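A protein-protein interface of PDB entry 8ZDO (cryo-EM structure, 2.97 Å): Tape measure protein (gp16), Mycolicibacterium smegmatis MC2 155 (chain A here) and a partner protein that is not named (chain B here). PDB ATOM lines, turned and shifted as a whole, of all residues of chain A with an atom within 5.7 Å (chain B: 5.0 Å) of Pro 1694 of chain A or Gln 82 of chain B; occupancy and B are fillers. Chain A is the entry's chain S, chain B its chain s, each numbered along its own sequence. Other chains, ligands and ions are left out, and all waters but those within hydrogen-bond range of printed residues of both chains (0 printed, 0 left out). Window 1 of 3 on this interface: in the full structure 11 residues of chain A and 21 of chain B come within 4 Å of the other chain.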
ATOM      1  N   ALA A1689      27.505   0.038  15.753  1.00  0.00           N
ATOM      2  CA  ALA A1689      26.956  -0.766  16.835  1.00  0.00           C
ATOM      3  C   ALA A1689      26.619   0.093  18.044  1.00  0.00           C
ATOM      4  O   ALA A1689      25.609  -0.140  18.712  1.00  0.00           O
ATOM      5  CB  ALA A1689      27.940  -1.869  17.218  1.00  0.00           C
ATOM      6  N   GLN A1690      27.461   1.079  18.349  1.00  0.00           N
ATOM      7  CA  GLN A1690      27.145   2.007  19.426  1.00  0.00           C
ATOM      8  C   GLN A1690      25.883   2.792  19.108  1.00  0.00           C
ATOM      9  O   GLN A1690      25.043   3.018  19.985  1.00  0.00           O
ATOM     10  CB  GLN A1690      28.321   2.953  19.663  1.00  0.00           C
ATOM     11  CG  GLN A1690      28.032   4.065  20.647  1.00  0.00           C
ATOM     12  CD  GLN A1690      29.290   4.763  21.109  1.00  0.00           C
ATOM     13  OE1 GLN A1690      30.392   4.414  20.693  1.00  0.00           O
ATOM     14  NE2 GLN A1690      29.132   5.755  21.973  1.00  0.00           N
ATOM     15  N   GLN A1691      25.735   3.217  17.853  1.00  0.00           N
ATOM     16  CA  GLN A1691      24.555   3.985  17.472  1.00  0.00           C
ATOM     17  C   GLN A1691      23.280   3.151  17.557  1.00  0.00           C
ATOM     18  O   GLN A1691      22.251   3.634  18.041  1.00  0.00           O
ATOM     19  CB  GLN A1691      24.731   4.547  16.064  1.00  0.00           C
ATOM     20  CG  GLN A1691      23.609   5.468  15.623  1.00  0.00           C
ATOM     21  CD  GLN A1691      23.589   6.767  16.398  1.00  0.00           C
ATOM     22  OE1 GLN A1691      24.632   7.267  16.822  1.00  0.00           O
ATOM     23  NE2 GLN A1691      22.398   7.321  16.593  1.00  0.00           N
ATOM     24  N   GLN A1692      23.325   1.899  17.099  1.00  0.00           N
ATOM     25  CA  GLN A1692      22.102   1.132  16.872  1.00  0.00           C
ATOM     26  C   GLN A1692      21.791   0.096  17.943  1.00  0.00           C
ATOM     27  O   GLN A1692      20.645  -0.357  18.020  1.00  0.00           O
ATOM     28  CB  GLN A1692      22.174   0.421  15.517  1.00  0.00           C
ATOM     29  CG  GLN A1692      22.155   1.361  14.332  1.00  0.00           C
ATOM     30  CD  GLN A1692      23.119   0.944  13.246  1.00  0.00           C
ATOM     31  OE1 GLN A1692      23.177  -0.225  12.868  1.00  0.00           O
ATOM     32  NE2 GLN A1692      23.886   1.900  12.736  1.00  0.00           N
ATOM     33  N   ALA A1693      22.765  -0.305  18.754  1.00  0.00           N
ATOM     34  CA  ALA A1693      22.529  -1.370  19.729  1.00  0.00           C
ATOM     35  C   ALA A1693      21.481  -1.016  20.775  1.00  0.00           C
ATOM     36  O   ALA A1693      20.597  -1.851  21.034  1.00  0.00           O
ATOM     37  CB  ALA A1693      23.855  -1.770  20.380  1.00  0.00           C
ATOM     38  N   PRO A1694      21.510   0.156  21.424  1.00  0.00           N
ATOM     39  CA  PRO A1694      20.487   0.435  22.446  1.00  0.00           C
ATOM     40  C   PRO A1694      19.067   0.442  21.909  1.00  0.00           C
ATOM     41  O   PRO A1694      18.138   0.088  22.645  1.00  0.00           O
ATOM     42  CB  PRO A1694      20.897   1.813  22.984  1.00  0.00           C
ATOM     43  CG  PRO A1694      21.708   2.412  21.902  1.00  0.00           C
ATOM     44  CD  PRO A1694      22.467   1.272  21.320  1.00  0.00           C
ATOM     45  N   ILE A1695      18.860   0.836  20.649  1.00  0.00           N
ATOM     46  CA  ILE A1695      17.509   0.913  20.102  1.00  0.00           C
ATOM     47  C   ILE A1695      17.045  -0.395  19.479  1.00  0.00           C
ATOM     48  O   ILE A1695      15.871  -0.500  19.091  1.00  0.00           O
ATOM     49  CB  ILE A1695      17.400   2.049  19.067  1.00  0.00           C
ATOM     50  CG1 ILE A1695      18.213   1.721  17.819  1.00  0.00           C
ATOM     51  CG2 ILE A1695      17.870   3.359  19.672  1.00  0.00           C
ATOM     52  CD1 ILE A1695      18.237   2.838  16.806  1.00  0.00           C
ATOM     53  N   LEU A1696      17.916  -1.389  19.366  1.00  0.00           N
ATOM     54  CA  LEU A1696      17.487  -2.688  18.872  1.00  0.00           C
ATOM     55  C   LEU A1696      16.669  -3.411  19.940  1.00  0.00           C
ATOM     56  O   LEU A1696      17.049  -3.417  21.116  1.00  0.00           O
ATOM     57  CB  LEU A1696      18.690  -3.536  18.468  1.00  0.00           C
ATOM     58  CG  LEU A1696      19.152  -3.363  17.023  1.00  0.00           C
ATOM     59  CD1 LEU A1696      20.381  -4.208  16.752  1.00  0.00           C
ATOM     60  CD2 LEU A1696      18.035  -3.715  16.058  1.00  0.00           C
ATOM     61  N   SER B  72      33.750   7.319  24.643  1.00  0.00           N
ATOM     62  CA  SER B  72      32.672   7.890  23.844  1.00  0.00           C
ATOM     63  C   SER B  72      31.394   7.833  24.663  1.00  0.00           C
ATOM     64  O   SER B  72      30.927   6.746  25.003  1.00  0.00           O
ATOM     65  CB  SER B  72      32.504   7.135  22.527  1.00  0.00           C
ATOM     66  OG  SER B  72      31.328   7.541  21.855  1.00  0.00           O
ATOM     67  N   PRO B  74      27.558   9.526  24.567  1.00  0.00           N
ATOM     68  CA  PRO B  74      26.545  10.406  23.977  1.00  0.00           C
ATOM     69  C   PRO B  74      25.385  10.706  24.912  1.00  0.00           C
ATOM     70  O   PRO B  74      24.966   9.851  25.697  1.00  0.00           O
ATOM     71  CB  PRO B  74      26.079   9.617  22.751  1.00  0.00           C
ATOM     72  CG  PRO B  74      26.379   8.173  23.074  1.00  0.00           C
ATOM     73  CD  PRO B  74      27.309   8.111  24.253  1.00  0.00           C
ATOM     74  N   PRO B  80      17.827   6.094  24.431  1.00  0.00           N
ATOM     75  CA  PRO B  80      18.957   5.428  25.082  1.00  0.00           C
ATOM     76  C   PRO B  80      20.202   5.477  24.215  1.00  0.00           C
ATOM     77  O   PRO B  80      20.131   5.512  22.985  1.00  0.00           O
ATOM     78  CB  PRO B  80      18.465   3.989  25.267  1.00  0.00           C
ATOM     79  CG  PRO B  80      16.984   4.067  25.149  1.00  0.00           C
ATOM     80  CD  PRO B  80      16.711   5.169  24.185  1.00  0.00           C
ATOM     81  N   SER B  81      21.356   5.477  24.874  1.00  0.00           N
ATOM     82  CA  SER B  81      22.634   5.546  24.184  1.00  0.00           C
ATOM     83  C   SER B  81      23.643   4.663  24.900  1.00  0.00           C
ATOM     84  O   SER B  81      23.503   4.352  26.084  1.00  0.00           O
ATOM     85  CB  SER B  81      23.147   6.988  24.097  1.00  0.00           C
ATOM     86  OG  SER B  81      23.282   7.561  25.385  1.00  0.00           O
ATOM     87  N   GLN B  82      24.670   4.261  24.158  1.00  0.00           N
ATOM     88  CA  GLN B  82      25.718   3.383  24.654  1.00  0.00           C
ATOM     89  C   GLN B  82      27.009   4.169  24.815  1.00  0.00           C
ATOM     90  O   GLN B  82      27.455   4.835  23.877  1.00  0.00           O
ATOM     91  CB  GLN B  82      25.941   2.208  23.702  1.00  0.00           C
ATOM     92  CG  GLN B  82      25.092   0.993  23.994  1.00  0.00           C
ATOM     93  CD  GLN B  82      25.592  -0.243  23.277  1.00  0.00           C
ATOM     94  OE1 GLN B  82      26.512  -0.173  22.464  1.00  0.00           O
ATOM     95  NE2 GLN B  82      24.989  -1.384  23.580  1.00  0.00           N
ATOM     96  N   GLY B  83      27.605   4.081  26.000  1.00  0.00           N
ATOM     97  CA  GLY B  83      28.890   4.699  26.267  1.00  0.00           C
ATOM     98  C   GLY B  83      29.982   3.646  26.293  1.00  0.00           C
ATOM     99  O   GLY B  83      29.838   2.605  26.931  1.00  0.00           O
ATOM    100  N   VAL B  84      31.075   3.933  25.598  1.00  0.00           N
ATOM    101  CA  VAL B  84      32.168   2.984  25.428  1.00  0.00           C
ATOM    102  C   VAL B  84      33.419   3.551  26.077  1.00  0.00           C
ATOM    103  O   VAL B  84      33.800   4.694  25.810  1.00  0.00           O
ATOM    104  CB  VAL B  84      32.419   2.669  23.944  1.00  0.00           C
ATOM    105  CG1 VAL B  84      33.328   1.463  23.813  1.00  0.00           C
ATOM    106  CG2 VAL B  84      31.108   2.428  23.230  1.00  0.00           C
ATOM    107  N   TRP B 123      27.004  11.686  32.904  1.00  0.00           N
ATOM    108  CA  TRP B 123      26.574  10.520  32.143  1.00  0.00           C
ATOM    109  C   TRP B 123      26.676   9.308  33.060  1.00  0.00           C
ATOM    110  O   TRP B 123      27.778   8.900  33.429  1.00  0.00           O
ATOM    111  CB  TRP B 123      27.434  10.334  30.895  1.00  0.00           C
ATOM    112  CG  TRP B 123      26.836   9.412  29.882  1.00  0.00           C
ATOM    113  CD1 TRP B 123      26.196   9.767  28.737  1.00  0.00           C
ATOM    114  CD2 TRP B 123      26.830   7.980  29.917  1.00  0.00           C
ATOM    115  NE1 TRP B 123      25.784   8.650  28.058  1.00  0.00           N
ATOM    116  CE2 TRP B 123      26.162   7.538  28.764  1.00  0.00           C
ATOM    117  CE3 TRP B 123      27.322   7.030  30.816  1.00  0.00           C
ATOM    118  CZ2 TRP B 123      25.972   6.190  28.483  1.00  0.00           C
ATOM    119  CZ3 TRP B 123      27.131   5.696  30.538  1.00  0.00           C
ATOM    120  CH2 TRP B 123      26.463   5.287  29.381  1.00  0.00           C
ATOM    121  N   ASP B 128      26.663  -2.677  30.275  1.00  0.00           N
ATOM    122  CA  ASP B 128      26.053  -3.591  29.320  1.00  0.00           C
ATOM    123  C   ASP B 128      26.906  -4.838  29.146  1.00  0.00           C
ATOM    124  O   ASP B 128      26.412  -5.962  29.286  1.00  0.00           O
ATOM    125  CB  ASP B 128      25.841  -2.893  27.977  1.00  0.00           C
ATOM    126  CG  ASP B 128      25.212  -3.799  26.941  1.00  0.00           C
ATOM    127  OD1 ASP B 128      24.405  -4.672  27.323  1.00  0.00           O
ATOM    128  OD2 ASP B 128      25.525  -3.642  25.744  1.00  0.00           O
ATOM    129  N   THR B 144      31.176  -1.479  27.584  1.00  0.00           N
ATOM    130  CA  THR B 144      29.992  -0.828  27.056  1.00  0.00           C
ATOM    131  C   THR B 144      28.959  -0.700  28.164  1.00  0.00           C
ATOM    132  O   THR B 144      28.600  -1.700  28.800  1.00  0.00           O
ATOM    133  CB  THR B 144      29.412  -1.623  25.886  1.00  0.00           C
ATOM    134  OG1 THR B 144      30.383  -1.708  24.837  1.00  0.00           O
ATOM    135  CG2 THR B 144      28.166  -0.954  25.361  1.00  0.00           C
ATOM    136  N   PHE B 145      28.502   0.528  28.389  1.00  0.00           N
ATOM    137  CA  PHE B 145      27.460   0.867  29.342  1.00  0.00           C
ATOM    138  C   PHE B 145      26.238   1.376  28.594  1.00  0.00           C
ATOM    139  O   PHE B 145      26.353   1.962  27.516  1.00  0.00           O
ATOM    140  CB  PHE B 145      27.918   1.951  30.324  1.00  0.00           C
ATOM    141  CG  PHE B 145      29.142   1.592  31.113  1.00  0.00           C
ATOM    142  CD1 PHE B 145      30.402   1.834  30.608  1.00  0.00           C
ATOM    143  CD2 PHE B 145      29.027   1.039  32.374  1.00  0.00           C
ATOM    144  CE1 PHE B 145      31.523   1.513  31.336  1.00  0.00           C
ATOM    145  CE2 PHE B 145      30.144   0.714  33.104  1.00  0.00           C
ATOM    146  CZ  PHE B 145      31.392   0.954  32.587  1.00  0.00           C
ATOM    147  N   ASN B 146      25.067   1.162  29.179  1.00  0.00           N
ATOM    148  CA  ASN B 146      23.821   1.709  28.666  1.00  0.00           C
ATOM    149  C   ASN B 146      23.377   2.841  29.579  1.00  0.00           C
ATOM    150  O   ASN B 146      23.300   2.660  30.796  1.00  0.00           O
ATOM    151  CB  ASN B 146      22.735   0.635  28.593  1.00  0.00           C
ATOM    152  CG  ASN B 146      22.970  -0.354  27.478  1.00  0.00           C
ATOM    153  OD1 ASN B 146      23.912  -0.219  26.704  1.00  0.00           O
ATOM    154  ND2 ASN B 146      22.108  -1.356  27.388  1.00  0.00           N
ATOM    155  N   GLN B 153      12.802   1.149  29.147  1.00  0.00           N
ATOM    156  CA  GLN B 153      12.493   0.016  28.283  1.00  0.00           C
ATOM    157  C   GLN B 153      12.047  -1.189  29.099  1.00  0.00           C
ATOM    158  O   GLN B 153      11.162  -1.940  28.676  1.00  0.00           O
ATOM    159  CB  GLN B 153      13.703  -0.345  27.427  1.00  0.00           C
ATOM    160  CG  GLN B 153      14.230   0.787  26.577  1.00  0.00           C
ATOM    161  CD  GLN B 153      15.421   0.372  25.745  1.00  0.00           C
ATOM    162  OE1 GLN B 153      16.189  -0.506  26.137  1.00  0.00           O
ATOM    163  NE2 GLN B 153      15.581   0.997  24.586  1.00  0.00           N
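The side-chain hydroxyl (OG) of Ser 81 of chain B is in hydrogen-bond range of the backbone carbonyl oxygen (O) of Pro 74 of chain B (2.9 Å). The backbone NH (N) of Ser 72 of chain B is in hydrogen-bond range of the backbone carbonyl oxygen (O) of Val 84 of chain B (2.9 Å). The indole nitrogen (NE1) of Trp 123 of chain B lies within hydrogen-bond range of the backbone carbonyl oxygen (O) of Pro 74 of chain B (2.8 Å). The side-chain amide nitrogen (NE2) of Gln 82 of chain B is in hydrogen-bond range of the side-chain carboxylate (OD2) of Asp 128 of chain B, 3.2 Å away.
NE2 of Gln 1690 of chain A lies within hydrogen-bond range of O of Gln 82 of chain B, at 2.7 Å. NE2 of Gln 1690 of chain A sits at hydrogen-bond distance from OG of Ser 72 of chain B. The side-chain amide nitrogen (NE2) of Gln 153 of chain B is in hydrogen-bond range of the backbone carbonyl oxygen (O) of Pro 1694 of chain A, 3.3 Å away.
Printed residues of chain B that touch a printed residue of chain A: Ser 72, Pro 74, Pro 80, Ser 81, Gln 82, Val 84 and Gln 153. Hydrophobic or aromatic side chains of chain B within 4 Å of the printed part of chain A: Pro 74, Pro 80 and Val 84. Of the 8 printed residues of chain A, 4 touch a printed residue of chain B. Hydrophobic or aromatic side chains of chain A that line the printed part of chain B: Ala 1693 and Pro 1694. Among the printed residues, 10 pairs touch across the chains.
Of the printed residues of chain B, Ala 1693 of chain A touches Gln 82. Printed residues of chain B within 4 Å of Pro 1694 of chain A: Pro 80 (3.6 Å), Ser 81 (3.99 Å), Gln 82 (3.8 Å) and Gln 153 (3.3 Å). Printed residues of chain A within 4 Å of Pro 80 of chain B: Pro 1694 (3.6 Å). Of the printed residues of chain A, Ser 81 of chain B touches Pro 1694 (3.99 Å). Of chain A, only Ala 1689, Gln 1690, Ala 1693 and Pro 1694 come within 4 Å of Gln 82 of chain B. Of the printed residues of chain A, Gln 153 of chain B touches Pro 1694 (3.3 Å). The nearest printed residue of chain B that does not touch Pro 1694 of chain A is Asn 146 of chain B (5.2 Å). The nearest printed residue of chain A that does not touch Ser 81 of chain B is Gln 1690 of chain A (5.4 Å).
Among the printed residues, merely in contact across the chains: Gln 1690 of chain A with Val 84 of chain B, Ala 1693 of chain A with Gln 82 of chain B, Pro 1694 of chain A with Pro 80 of chain B, Gln 1690 of chain A with Pro 74 of chain B, Pro 1694 of chain A with Gln 82 of chain B, Ala 1689 of chain A with Gln 82 of chain B and Pro 1694 of chain A with Ser 81 of chain B.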
